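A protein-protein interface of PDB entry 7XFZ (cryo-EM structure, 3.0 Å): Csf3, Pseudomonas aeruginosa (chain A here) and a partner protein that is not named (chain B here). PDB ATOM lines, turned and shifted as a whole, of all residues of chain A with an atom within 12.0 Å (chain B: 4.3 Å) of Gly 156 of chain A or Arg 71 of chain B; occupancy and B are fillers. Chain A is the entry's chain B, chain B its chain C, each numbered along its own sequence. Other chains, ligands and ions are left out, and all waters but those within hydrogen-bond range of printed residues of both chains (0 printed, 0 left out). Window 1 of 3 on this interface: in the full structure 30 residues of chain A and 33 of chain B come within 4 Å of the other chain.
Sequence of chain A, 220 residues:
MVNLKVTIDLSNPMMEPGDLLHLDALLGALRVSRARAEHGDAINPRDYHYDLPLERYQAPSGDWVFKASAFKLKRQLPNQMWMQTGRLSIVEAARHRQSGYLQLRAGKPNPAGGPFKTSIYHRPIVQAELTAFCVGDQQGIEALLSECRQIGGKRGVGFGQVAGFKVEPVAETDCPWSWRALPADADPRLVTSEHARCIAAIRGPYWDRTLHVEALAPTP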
ATOM      1  N   ASN A  12     -23.849 -21.502  15.797  1.00  0.00           N
ATOM      2  CA  ASN A  12     -24.438 -20.186  15.608  1.00  0.00           C
ATOM      3  C   ASN A  12     -25.307 -20.235  14.367  1.00  0.00           C
ATOM      4  O   ASN A  12     -24.920 -20.863  13.375  1.00  0.00           O
ATOM      5  CB  ASN A  12     -23.346 -19.119  15.453  1.00  0.00           C
ATOM      6  CG  ASN A  12     -23.767 -17.772  15.978  1.00  0.00           C
ATOM      7  OD1 ASN A  12     -23.479 -16.744  15.371  1.00  0.00           O
ATOM      8  ND2 ASN A  12     -24.440 -17.766  17.120  1.00  0.00           N
ATOM      9  N   PRO A  13     -26.483 -19.613  14.388  1.00  0.00           N
ATOM     10  CA  PRO A  13     -27.272 -19.510  13.157  1.00  0.00           C
ATOM     11  C   PRO A  13     -26.494 -18.770  12.079  1.00  0.00           C
ATOM     12  O   PRO A  13     -25.772 -17.811  12.356  1.00  0.00           O
ATOM     13  CB  PRO A  13     -28.515 -18.731  13.597  1.00  0.00           C
ATOM     14  CG  PRO A  13     -28.626 -19.010  15.050  1.00  0.00           C
ATOM     15  CD  PRO A  13     -27.218 -19.103  15.556  1.00  0.00           C
ATOM     16  N   MET A  14     -26.645 -19.228  10.841  1.00  0.00           N
ATOM     17  CA  MET A  14     -25.937 -18.655   9.710  1.00  0.00           C
ATOM     18  C   MET A  14     -26.935 -18.152   8.682  1.00  0.00           C
ATOM     19  O   MET A  14     -28.083 -18.597   8.637  1.00  0.00           O
ATOM     20  CB  MET A  14     -24.995 -19.672   9.061  1.00  0.00           C
ATOM     21  CG  MET A  14     -25.698 -20.730   8.238  1.00  0.00           C
ATOM     22  SD  MET A  14     -24.609 -21.518   7.040  1.00  0.00           S
ATOM     23  CE  MET A  14     -25.777 -22.544   6.161  1.00  0.00           C
ATOM     24  N   MET A  15     -26.489 -17.201   7.866  1.00  0.00           N
ATOM     25  CA  MET A  15     -27.314 -16.710   6.773  1.00  0.00           C
ATOM     26  C   MET A  15     -27.597 -17.834   5.787  1.00  0.00           C
ATOM     27  O   MET A  15     -26.677 -18.513   5.323  1.00  0.00           O
ATOM     28  CB  MET A  15     -26.614 -15.553   6.064  1.00  0.00           C
ATOM     29  CG  MET A  15     -26.565 -14.255   6.841  1.00  0.00           C
ATOM     30  SD  MET A  15     -27.900 -13.132   6.401  1.00  0.00           S
ATOM     31  CE  MET A  15     -28.633 -12.819   7.998  1.00  0.00           C
ATOM     32  N   TRP A  82     -34.332 -12.310   9.787  1.00  0.00           N
ATOM     33  CA  TRP A  82     -33.453 -11.364  10.465  1.00  0.00           C
ATOM     34  C   TRP A  82     -33.537 -10.009   9.780  1.00  0.00           C
ATOM     35  O   TRP A  82     -33.492  -9.933   8.550  1.00  0.00           O
ATOM     36  CB  TRP A  82     -32.008 -11.877  10.460  1.00  0.00           C
ATOM     37  CG  TRP A  82     -31.062 -11.109  11.326  1.00  0.00           C
ATOM     38  CD1 TRP A  82     -30.100 -10.241  10.914  1.00  0.00           C
ATOM     39  CD2 TRP A  82     -30.961 -11.169  12.753  1.00  0.00           C
ATOM     40  NE1 TRP A  82     -29.417  -9.741  11.992  1.00  0.00           N
ATOM     41  CE2 TRP A  82     -29.926 -10.296  13.134  1.00  0.00           C
ATOM     42  CE3 TRP A  82     -31.652 -11.869  13.745  1.00  0.00           C
ATOM     43  CZ2 TRP A  82     -29.565 -10.104  14.463  1.00  0.00           C
ATOM     44  CZ3 TRP A  82     -31.290 -11.678  15.063  1.00  0.00           C
ATOM     45  CH2 TRP A  82     -30.257 -10.804  15.410  1.00  0.00           C
ATOM     46  N   GLN A  84     -32.152  -5.937   9.439  1.00  0.00           N
ATOM     47  CA  GLN A  84     -31.070  -4.988   9.646  1.00  0.00           C
ATOM     48  C   GLN A  84     -31.444  -3.666   8.995  1.00  0.00           C
ATOM     49  O   GLN A  84     -32.307  -3.605   8.119  1.00  0.00           O
ATOM     50  CB  GLN A  84     -29.742  -5.510   9.091  1.00  0.00           C
ATOM     51  CG  GLN A  84     -29.105  -6.582   9.950  1.00  0.00           C
ATOM     52  CD  GLN A  84     -27.752  -7.017   9.439  1.00  0.00           C
ATOM     53  OE1 GLN A  84     -27.320  -6.606   8.366  1.00  0.00           O
ATOM     54  NE2 GLN A  84     -27.077  -7.859  10.205  1.00  0.00           N
ATOM     55  N   THR A  85     -30.792  -2.597   9.443  1.00  0.00           N
ATOM     56  CA  THR A  85     -31.144  -1.245   9.038  1.00  0.00           C
ATOM     57  C   THR A  85     -29.878  -0.469   8.700  1.00  0.00           C
ATOM     58  O   THR A  85     -28.837  -0.667   9.329  1.00  0.00           O
ATOM     59  CB  THR A  85     -31.940  -0.537  10.155  1.00  0.00           C
ATOM     60  OG1 THR A  85     -33.298  -0.989  10.138  1.00  0.00           O
ATOM     61  CG2 THR A  85     -31.932   0.966   9.988  1.00  0.00           C
ATOM     62  N   GLY A  86     -29.964   0.393   7.692  1.00  0.00           N
ATOM     63  CA  GLY A  86     -28.890   1.321   7.397  1.00  0.00           C
ATOM     64  C   GLY A  86     -29.346   2.763   7.469  1.00  0.00           C
ATOM     65  O   GLY A  86     -30.308   3.143   6.799  1.00  0.00           O
ATOM     66  N   ARG A  87     -28.669   3.579   8.275  1.00  0.00           N
ATOM     67  CA  ARG A  87     -29.068   4.968   8.462  1.00  0.00           C
ATOM     68  C   ARG A  87     -27.844   5.814   8.784  1.00  0.00           C
ATOM     69  O   ARG A  87     -26.890   5.321   9.391  1.00  0.00           O
ATOM     70  CB  ARG A  87     -30.117   5.087   9.575  1.00  0.00           C
ATOM     71  CG  ARG A  87     -29.573   5.518  10.922  1.00  0.00           C
ATOM     72  CD  ARG A  87     -30.682   5.658  11.955  1.00  0.00           C
ATOM     73  NE  ARG A  87     -31.281   4.374  12.297  1.00  0.00           N
ATOM     74  CZ  ARG A  87     -32.570   4.091  12.175  1.00  0.00           C
ATOM     75  NH1 ARG A  87     -33.434   4.983  11.721  1.00  0.00           N
ATOM     76  NH2 ARG A  87     -33.005   2.884  12.522  1.00  0.00           N
ATOM     77  N   TYR A 121     -33.911  -3.961   5.469  1.00  0.00           N
ATOM     78  CA  TYR A 121     -33.809  -5.162   4.655  1.00  0.00           C
ATOM     79  C   TYR A 121     -33.828  -6.383   5.562  1.00  0.00           C
ATOM     80  O   TYR A 121     -33.342  -6.340   6.693  1.00  0.00           O
ATOM     81  CB  TYR A 121     -32.546  -5.156   3.778  1.00  0.00           C
ATOM     82  CG  TYR A 121     -31.249  -4.934   4.524  1.00  0.00           C
ATOM     83  CD1 TYR A 121     -30.858  -3.664   4.914  1.00  0.00           C
ATOM     84  CD2 TYR A 121     -30.412  -5.996   4.827  1.00  0.00           C
ATOM     85  CE1 TYR A 121     -29.677  -3.460   5.590  1.00  0.00           C
ATOM     86  CE2 TYR A 121     -29.230  -5.800   5.503  1.00  0.00           C
ATOM     87  CZ  TYR A 121     -28.868  -4.530   5.882  1.00  0.00           C
ATOM     88  OH  TYR A 121     -27.689  -4.328   6.557  1.00  0.00           O
ATOM     89  N   ARG A 123     -33.434 -10.815   5.860  1.00  0.00           N
ATOM     90  CA  ARG A 123     -32.791 -12.014   5.334  1.00  0.00           C
ATOM     91  C   ARG A 123     -33.057 -13.184   6.270  1.00  0.00           C
ATOM     92  O   ARG A 123     -33.055 -12.998   7.494  1.00  0.00           O
ATOM     93  CB  ARG A 123     -31.280 -11.827   5.171  1.00  0.00           C
ATOM     94  CG  ARG A 123     -30.871 -10.741   4.193  1.00  0.00           C
ATOM     95  CD  ARG A 123     -30.057 -11.303   3.041  1.00  0.00           C
ATOM     96  NE  ARG A 123     -28.815 -11.920   3.492  1.00  0.00           N
ATOM     97  CZ  ARG A 123     -27.834 -12.304   2.687  1.00  0.00           C
ATOM     98  NH1 ARG A 123     -27.908 -12.138   1.377  1.00  0.00           N
ATOM     99  NH2 ARG A 123     -26.748 -12.869   3.211  1.00  0.00           N
ATOM    100  N   ARG A 149     -13.143 -20.860   9.989  1.00  0.00           N
ATOM    101  CA  ARG A 149     -13.806 -20.572  11.251  1.00  0.00           C
ATOM    102  C   ARG A 149     -15.194 -19.964  11.099  1.00  0.00           C
ATOM    103  O   ARG A 149     -15.884 -19.792  12.109  1.00  0.00           O
ATOM    104  CB  ARG A 149     -12.939 -19.635  12.103  1.00  0.00           C
ATOM    105  CG  ARG A 149     -12.773 -18.256  11.507  1.00  0.00           C
ATOM    106  CD  ARG A 149     -11.833 -17.402  12.332  1.00  0.00           C
ATOM    107  NE  ARG A 149     -11.695 -16.052  11.800  1.00  0.00           N
ATOM    108  CZ  ARG A 149     -10.873 -15.720  10.815  1.00  0.00           C
ATOM    109  NH1 ARG A 149     -10.091 -16.617  10.235  1.00  0.00           N
ATOM    110  NH2 ARG A 149     -10.834 -14.457  10.399  1.00  0.00           N
ATOM    111  N   GLN A 150     -15.617 -19.622   9.885  1.00  0.00           N
ATOM    112  CA  GLN A 150     -16.972 -19.145   9.648  1.00  0.00           C
ATOM    113  C   GLN A 150     -17.442 -19.661   8.298  1.00  0.00           C
ATOM    114  O   GLN A 150     -16.635 -19.905   7.397  1.00  0.00           O
ATOM    115  CB  GLN A 150     -17.058 -17.618   9.683  1.00  0.00           C
ATOM    116  CG  GLN A 150     -17.568 -17.057  10.993  1.00  0.00           C
ATOM    117  CD  GLN A 150     -17.195 -15.609  11.183  1.00  0.00           C
ATOM    118  OE1 GLN A 150     -16.059 -15.288  11.520  1.00  0.00           O
ATOM    119  NE2 GLN A 150     -18.155 -14.722  10.979  1.00  0.00           N
ATOM    120  N   ILE A 151     -18.753 -19.824   8.161  1.00  0.00           N
ATOM    121  CA  ILE A 151     -19.343 -20.311   6.920  1.00  0.00           C
ATOM    122  C   ILE A 151     -20.581 -19.482   6.605  1.00  0.00           C
ATOM    123  O   ILE A 151     -21.347 -19.122   7.504  1.00  0.00           O
ATOM    124  CB  ILE A 151     -19.667 -21.818   7.002  1.00  0.00           C
ATOM    125  CG1 ILE A 151     -20.110 -22.348   5.638  1.00  0.00           C
ATOM    126  CG2 ILE A 151     -20.714 -22.099   8.064  1.00  0.00           C
ATOM    127  CD1 ILE A 151     -20.104 -23.847   5.541  1.00  0.00           C
ATOM    128  N   GLY A 152     -20.757 -19.154   5.330  1.00  0.00           N
ATOM    129  CA  GLY A 152     -21.896 -18.376   4.881  1.00  0.00           C
ATOM    130  C   GLY A 152     -21.547 -16.917   4.663  1.00  0.00           C
ATOM    131  O   GLY A 152     -20.386 -16.499   4.683  1.00  0.00           O
ATOM    132  N   GLY A 153     -22.599 -16.129   4.437  1.00  0.00           N
ATOM    133  CA  GLY A 153     -22.458 -14.703   4.247  1.00  0.00           C
ATOM    134  C   GLY A 153     -22.628 -13.925   5.538  1.00  0.00           C
ATOM    135  O   GLY A 153     -22.925 -14.472   6.598  1.00  0.00           O
ATOM    136  N   LYS A 154     -22.438 -12.612   5.425  1.00  0.00           N
ATOM    137  CA  LYS A 154     -22.531 -11.686   6.552  1.00  0.00           C
ATOM    138  C   LYS A 154     -21.603 -12.111   7.687  1.00  0.00           C
ATOM    139  O   LYS A 154     -21.966 -12.105   8.862  1.00  0.00           O
ATOM    140  CB  LYS A 154     -23.975 -11.559   7.038  1.00  0.00           C
ATOM    141  CG  LYS A 154     -24.893 -10.845   6.065  1.00  0.00           C
ATOM    142  CD  LYS A 154     -24.459  -9.410   5.851  1.00  0.00           C
ATOM    143  CE  LYS A 154     -25.413  -8.675   4.923  1.00  0.00           C
ATOM    144  NZ  LYS A 154     -24.932  -7.301   4.610  1.00  0.00           N
ATOM    145  N   ARG A 155     -20.378 -12.478   7.317  1.00  0.00           N
ATOM    146  CA  ARG A 155     -19.406 -12.954   8.290  1.00  0.00           C
ATOM    147  C   ARG A 155     -18.860 -11.843   9.174  1.00  0.00           C
ATOM    148  O   ARG A 155     -18.287 -12.141  10.226  1.00  0.00           O
ATOM    149  CB  ARG A 155     -18.257 -13.654   7.570  1.00  0.00           C
ATOM    150  CG  ARG A 155     -18.626 -15.010   7.004  1.00  0.00           C
ATOM    151  CD  ARG A 155     -17.438 -15.672   6.347  1.00  0.00           C
ATOM    152  NE  ARG A 155     -16.798 -14.814   5.358  1.00  0.00           N
ATOM    153  CZ  ARG A 155     -17.176 -14.720   4.091  1.00  0.00           C
ATOM    154  NH1 ARG A 155     -18.206 -15.405   3.627  1.00  0.00           N
ATOM    155  NH2 ARG A 155     -16.499 -13.925   3.270  1.00  0.00           N
ATOM    156  N   GLY A 156     -19.023 -10.581   8.782  1.00  0.00           N
ATOM    157  CA  GLY A 156     -18.506  -9.479   9.569  1.00  0.00           C
ATOM    158  C   GLY A 156     -19.328  -9.106  10.777  1.00  0.00           C
ATOM    159  O   GLY A 156     -18.868  -8.305  11.595  1.00  0.00           O
ATOM    160  N   VAL A 157     -20.530  -9.660  10.912  1.00  0.00           N
ATOM    161  CA  VAL A 157     -21.380  -9.416  12.068  1.00  0.00           C
ATOM    162  C   VAL A 157     -21.542 -10.678  12.915  1.00  0.00           C
ATOM    163  O   VAL A 157     -22.394 -10.732  13.791  1.00  0.00           O
ATOM    164  CB  VAL A 157     -22.749  -8.846  11.646  1.00  0.00           C
ATOM    165  CG1 VAL A 157     -22.610  -7.399  11.216  1.00  0.00           C
ATOM    166  CG2 VAL A 157     -23.348  -9.673  10.533  1.00  0.00           C
ATOM    167  N   GLY A 158     -20.729 -11.698  12.653  1.00  0.00           N
ATOM    168  CA  GLY A 158     -20.653 -12.860  13.511  1.00  0.00           C
ATOM    169  C   GLY A 158     -21.568 -14.013  13.171  1.00  0.00           C
ATOM    170  O   GLY A 158     -21.871 -14.815  14.061  1.00  0.00           O
ATOM    171  N   PHE A 159     -22.014 -14.134  11.925  1.00  0.00           N
ATOM    172  CA  PHE A 159     -22.931 -15.199  11.543  1.00  0.00           C
ATOM    173  C   PHE A 159     -22.172 -16.432  11.073  1.00  0.00           C
ATOM    174  O   PHE A 159     -21.278 -16.345  10.228  1.00  0.00           O
ATOM    175  CB  PHE A 159     -23.880 -14.724  10.441  1.00  0.00           C
ATOM    176  CG  PHE A 159     -25.096 -14.020  10.956  1.00  0.00           C
ATOM    177  CD1 PHE A 159     -26.043 -14.700  11.699  1.00  0.00           C
ATOM    178  CD2 PHE A 159     -25.290 -12.675  10.707  1.00  0.00           C
ATOM    179  CE1 PHE A 159     -27.158 -14.054  12.180  1.00  0.00           C
ATOM    180  CE2 PHE A 159     -26.403 -12.026  11.187  1.00  0.00           C
ATOM    181  CZ  PHE A 159     -27.337 -12.715  11.924  1.00  0.00           C
ATOM    182  N   GLY A 160     -22.537 -17.584  11.631  1.00  0.00           N
ATOM    183  CA  GLY A 160     -22.048 -18.861  11.154  1.00  0.00           C
ATOM    184  C   GLY A 160     -20.737 -19.326  11.749  1.00  0.00           C
ATOM    185  O   GLY A 160     -19.850 -19.771  11.018  1.00  0.00           O
ATOM    186  N   GLN A 161     -20.596 -19.240  13.067  1.00  0.00           N
ATOM    187  CA  GLN A 161     -19.394 -19.742  13.716  1.00  0.00           C
ATOM    188  C   GLN A 161     -19.403 -21.264  13.723  1.00  0.00           C
ATOM    189  O   GLN A 161     -20.388 -21.884  14.131  1.00  0.00           O
ATOM    190  CB  GLN A 161     -19.301 -19.214  15.145  1.00  0.00           C
ATOM    191  CG  GLN A 161     -19.921 -17.851  15.347  1.00  0.00           C
ATOM    192  CD  GLN A 161     -18.896 -16.741  15.319  1.00  0.00           C
ATOM    193  OE1 GLN A 161     -17.708 -16.973  15.528  1.00  0.00           O
ATOM    194  NE2 GLN A 161     -19.354 -15.524  15.063  1.00  0.00           N
ATOM    195  N   GLY B  67     -25.349  -7.628  16.206  1.00  0.00           N
ATOM    196  CA  GLY B  67     -23.951  -7.319  15.961  1.00  0.00           C
ATOM    197  C   GLY B  67     -23.741  -6.115  15.069  1.00  0.00           C
ATOM    198  O   GLY B  67     -22.688  -5.473  15.128  1.00  0.00           O
ATOM    199  N   ASN B  68     -24.725  -5.793  14.228  1.00  0.00           N
ATOM    200  CA  ASN B  68     -24.659  -4.565  13.443  1.00  0.00           C
ATOM    201  C   ASN B  68     -24.662  -3.342  14.351  1.00  0.00           C
ATOM    202  O   ASN B  68     -23.913  -2.384  14.124  1.00  0.00           O
ATOM    203  CB  ASN B  68     -25.828  -4.515  12.464  1.00  0.00           C
ATOM    204  CG  ASN B  68     -25.439  -3.958  11.113  1.00  0.00           C
ATOM    205  OD1 ASN B  68     -24.281  -4.030  10.708  1.00  0.00           O
ATOM    206  ND2 ASN B  68     -26.409  -3.401  10.404  1.00  0.00           N
ATOM    207  N   THR B  69     -25.492  -3.370  15.396  1.00  0.00           N
ATOM    208  CA  THR B  69     -25.535  -2.274  16.357  1.00  0.00           C
ATOM    209  C   THR B  69     -24.193  -2.096  17.058  1.00  0.00           C
ATOM    210  O   THR B  69     -23.703  -0.970  17.197  1.00  0.00           O
ATOM    211  CB  THR B  69     -26.646  -2.528  17.376  1.00  0.00           C
ATOM    212  OG1 THR B  69     -27.922  -2.329  16.757  1.00  0.00           O
ATOM    213  CG2 THR B  69     -26.518  -1.596  18.564  1.00  0.00           C
ATOM    214  N   MET B  70     -23.578  -3.195  17.498  1.00  0.00           N
ATOM    215  CA  MET B  70     -22.297  -3.103  18.193  1.00  0.00           C
ATOM    216  C   MET B  70     -21.185  -2.646  17.256  1.00  0.00           C
ATOM    217  O   MET B  70     -20.311  -1.863  17.652  1.00  0.00           O
ATOM    218  CB  MET B  70     -21.952  -4.448  18.828  1.00  0.00           C
ATOM    219  CG  MET B  70     -23.059  -5.031  19.692  1.00  0.00           C
ATOM    220  SD  MET B  70     -23.579  -3.920  21.009  1.00  0.00           S
ATOM    221  CE  MET B  70     -22.055  -3.726  21.924  1.00  0.00           C
ATOM    222  N   ARG B  71     -21.199  -3.126  16.012  1.00  0.00           N
ATOM    223  CA  ARG B  71     -20.218  -2.682  15.029  1.00  0.00           C
ATOM    224  C   ARG B  71     -20.330  -1.184  14.785  1.00  0.00           C
ATOM    225  O   ARG B  71     -19.320  -0.467  14.742  1.00  0.00           O
ATOM    226  CB  ARG B  71     -20.412  -3.462  13.730  1.00  0.00           C
ATOM    227  CG  ARG B  71     -19.371  -3.200  12.663  1.00  0.00           C
ATOM    228  CD  ARG B  71     -19.721  -3.954  11.394  1.00  0.00           C
ATOM    229  NE  ARG B  71     -18.764  -3.716  10.320  1.00  0.00           N
ATOM    230  CZ  ARG B  71     -17.738  -4.506  10.042  1.00  0.00           C
ATOM    231  NH1 ARG B  71     -17.489  -5.592  10.752  1.00  0.00           N
ATOM    232  NH2 ARG B  71     -16.941  -4.199   9.024  1.00  0.00           N
ATOM    233  N   SER B  72     -21.560  -0.685  14.640  1.00  0.00           N
ATOM    234  CA  SER B  72     -21.749   0.744  14.433  1.00  0.00           C
ATOM    235  C   SER B  72     -21.343   1.543  15.664  1.00  0.00           C
ATOM    236  O   SER B  72     -20.794   2.640  15.539  1.00  0.00           O
ATOM    237  CB  SER B  72     -23.197   1.036  14.058  1.00  0.00           C
ATOM    238  OG  SER B  72     -23.380   2.413  13.788  1.00  0.00           O
ATOM    239  N   LEU B  73     -21.611   1.017  16.861  1.00  0.00           N
ATOM    240  CA  LEU B  73     -21.192   1.703  18.080  1.00  0.00           C
ATOM    241  C   LEU B  73     -19.678   1.842  18.139  1.00  0.00           C
ATOM    242  O   LEU B  73     -19.156   2.915  18.466  1.00  0.00           O
ATOM    243  CB  LEU B  73     -21.706   0.953  19.307  1.00  0.00           C
ATOM    244  CG  LEU B  73     -21.197   1.435  20.666  1.00  0.00           C
ATOM    245  CD1 LEU B  73     -21.735   2.816  20.976  1.00  0.00           C
ATOM    246  CD2 LEU B  73     -21.566   0.456  21.765  1.00  0.00           C
ATOM    247  N   LEU B  74     -18.957   0.764  17.824  1.00  0.00           N
ATOM    248  CA  LEU B  74     -17.500   0.827  17.817  1.00  0.00           C
ATOM    249  C   LEU B  74     -16.994   1.819  16.775  1.00  0.00           C
ATOM    250  O   LEU B  74     -16.087   2.615  17.051  1.00  0.00           O
ATOM    251  CB  LEU B  74     -16.920  -0.564  17.568  1.00  0.00           C
ATOM    252  CG  LEU B  74     -15.401  -0.715  17.643  1.00  0.00           C
ATOM    253  CD1 LEU B  74     -14.936  -0.817  19.085  1.00  0.00           C
ATOM    254  CD2 LEU B  74     -14.959  -1.930  16.849  1.00  0.00           C
ATOM    255  N   ARG B  75     -17.583   1.799  15.576  1.00  0.00           N
ATOM    256  CA  ARG B  75     -17.172   2.741  14.537  1.00  0.00           C
ATOM    257  C   ARG B  75     -17.395   4.182  14.979  1.00  0.00           C
ATOM    258  O   ARG B  75     -16.524   5.041  14.799  1.00  0.00           O
ATOM    259  CB  ARG B  75     -17.935   2.456  13.244  1.00  0.00           C
ATOM    260  CG  ARG B  75     -17.511   3.317  12.076  1.00  0.00           C
ATOM    261  CD  ARG B  75     -18.638   3.482  11.080  1.00  0.00           C
ATOM    262  NE  ARG B  75     -18.894   2.260  10.330  1.00  0.00           N
ATOM    263  CZ  ARG B  75     -18.413   2.008   9.121  1.00  0.00           C
ATOM    264  NH1 ARG B  75     -17.633   2.870   8.495  1.00  0.00           N
ATOM    265  NH2 ARG B  75     -18.722   0.860   8.527  1.00  0.00           N
ATOM    266  N   PHE B 133     -12.687  -0.952   8.845  1.00  0.00           N
ATOM    267  CA  PHE B 133     -13.984  -1.015   8.188  1.00  0.00           C
ATOM    268  C   PHE B 133     -13.810  -0.683   6.713  1.00  0.00           C
ATOM    269  O   PHE B 133     -13.222   0.347   6.368  1.00  0.00           O
ATOM    270  CB  PHE B 133     -14.993  -0.036   8.806  1.00  0.00           C
ATOM    271  CG  PHE B 133     -14.984   0.000  10.308  1.00  0.00           C
ATOM    272  CD1 PHE B 133     -14.105   0.821  10.992  1.00  0.00           C
ATOM    273  CD2 PHE B 133     -15.877  -0.763  11.034  1.00  0.00           C
ATOM    274  CE1 PHE B 133     -14.102   0.860  12.369  1.00  0.00           C
ATOM    275  CE2 PHE B 133     -15.881  -0.725  12.408  1.00  0.00           C
ATOM    276  CZ  PHE B 133     -14.992   0.088  13.077  1.00  0.00           C
ATOM    277  N   LEU B 144     -12.410  -6.597  10.470  1.00  0.00           N
ATOM    278  CA  LEU B 144     -13.108  -6.673  11.743  1.00  0.00           C
ATOM    279  C   LEU B 144     -14.237  -7.689  11.681  1.00  0.00           C
ATOM    280  O   LEU B 144     -14.985  -7.745  10.700  1.00  0.00           O
ATOM    281  CB  LEU B 144     -13.674  -5.310  12.141  1.00  0.00           C
ATOM    282  CG  LEU B 144     -12.881  -4.530  13.182  1.00  0.00           C
ATOM    283  CD1 LEU B 144     -13.616  -3.264  13.553  1.00  0.00           C
ATOM    284  CD2 LEU B 144     -12.641  -5.388  14.402  1.00  0.00           C
ATOM    285  N   MET B 145     -14.353  -8.485  12.740  1.00  0.00           N
ATOM    286  CA  MET B 145     -15.489  -9.369  12.971  1.00  0.00           C
ATOM    287  C   MET B 145     -16.070  -8.997  14.326  1.00  0.00           C
ATOM    288  O   MET B 145     -15.438  -9.236  15.361  1.00  0.00           O
ATOM    289  CB  MET B 145     -15.062 -10.835  12.935  1.00  0.00           C
ATOM    290  CG  MET B 145     -16.193 -11.827  12.722  1.00  0.00           C
ATOM    291  SD  MET B 145     -17.226 -12.110  14.172  1.00  0.00           S
ATOM    292  CE  MET B 145     -16.024 -12.725  15.345  1.00  0.00           C
ATOM    293  N   VAL B 146     -17.262  -8.408  14.329  1.00  0.00           N
ATOM    294  CA  VAL B 146     -17.912  -7.951  15.551  1.00  0.00           C
ATOM    295  C   VAL B 146     -19.123  -8.834  15.810  1.00  0.00           C
ATOM    296  O   VAL B 146     -20.103  -8.794  15.057  1.00  0.00           O
ATOM    297  CB  VAL B 146     -18.319  -6.474  15.463  1.00  0.00           C
ATOM    298  CG1 VAL B 146     -18.623  -5.933  16.841  1.00  0.00           C
ATOM    299  CG2 VAL B 146     -17.214  -5.664  14.816  1.00  0.00           C
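Met 15 of chain A touches none of the printed residues of chain B. Of the printed residues of chain B, Thr 85 of chain A touches Asn 68 (3.8 Å). Of the printed residues of chain B, Arg 155 of chain A touches Met 145. Gly 156 of chain A touches just these residues of chain B: Arg 71 (3.2 Å), Met 145 (3.8 Å) and Val 146 (3.2 Å). Of the printed residues of chain B, Val 157 of chain A touches Asn 68 (3.8 Å) and Val 146 (3.2 Å). Asn 68 of chain B touches just these residues of chain A: Gln 84 (3.9 Å), Thr 85 (3.8 Å) and Val 157 (3.8 Å). No residue of chain A comes within 4 Å of Thr 69 of chain B. Printed residues of chain A within 4 Å of Arg 71 of chain B: Gly 156 (3.2 Å). No residue of chain A comes within 4 Å of Ser 72 of chain B. No residue of chain A comes within 4 Å of Leu 73 of chain B. No residue of chain A comes within 4 Å of Leu 74 of chain B. Phe 133 of chain B touches none of the printed residues of chain A. No residue of chain A comes within 4 Å of Leu 144 of chain B. Met 145 of chain B touches just these residues of chain A: Gln 150, Arg 155, Gly 156 and Gly 158. Val 146 of chain B touches just these residues of chain A: Gly 156 (3.2 Å), Val 157 (3.2 Å) and Gly 158 (3.8 Å). The nearest residue of chain B that does not touch Gly 156 of chain A is Leu 144 of chain B (4.02 Å). The nearest residue of chain A that does not touch Arg 71 of chain B is Val 157 of chain A (4.5 Å).
Hydrophobic or aromatic side chains of chain B that line the printed part of chain A: Met 145. Hydrophobic or aromatic side chains of chain A within 4 Å of the printed part of chain B: Val 157. Among the printed residues, 11 pairs touch across the chains. Among the printed residues, no Asp or Glu carboxylate lies within 4 Å of a Lys or Arg side-chain nitrogen of the other chain.
O of Val 157 of chain A sits close to O of Val 146 of chain B. The guanidinium group (NH1) of Arg 71 of chain B is in hydrogen-bond range of the backbone carbonyl oxygen (O) of Gly 156 of chain A (3.2 Å). The backbone carbonyl oxygen of Gly 156 of chain A is in hydrogen-bond range of the backbone NH of Val 146 of chain B (3.2 Å).
The side-chain amide nitrogen (NE2) of Gln 161 of chain A lies within hydrogen-bond range of the backbone carbonyl oxygen (O) of Gly 158 of chain A, at 2.8 Å. O of Gly 152 of chain A is in hydrogen-bond range of NH1 of Arg 155 of chain A (2.7 Å). The side-chain hydroxyl (OH) of Tyr 121 of chain A sits at hydrogen-bond distance from the side-chain amide oxygen (OE1) of Gln 84 of chain A. OD1 of Asn 12 of chain A lies close to O of Gly 158 of chain A, at 2.8 Å. The backbone carbonyl oxygen of Leu 144 of chain B sits at hydrogen-bond distance from the guanidinium group of Arg 71 of chain B, 3.3 Å away. The side-chain amide nitrogen (NE2) of Gln 84 of chain A sits close to the indole nitrogen (NE1) of Trp 82 of chain A (3.5 Å).
Among the printed residues, merely in contact across the chains: Arg 155 of chain A with Met 145 of chain B, Gly 158 of chain A with Met 145 of chain B, Gln 150 of chain A with Met 145 of chain B, Val 157 of chain A with Asn 68 of chain B, Gly 156 of chain A with Met 145 of chain B, Thr 85 of chain A with Asn 68 of chain B, Gly 158 of chain A with Val 146 of chain B and Gln 84 of chain A with Asn 68 of chain B.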
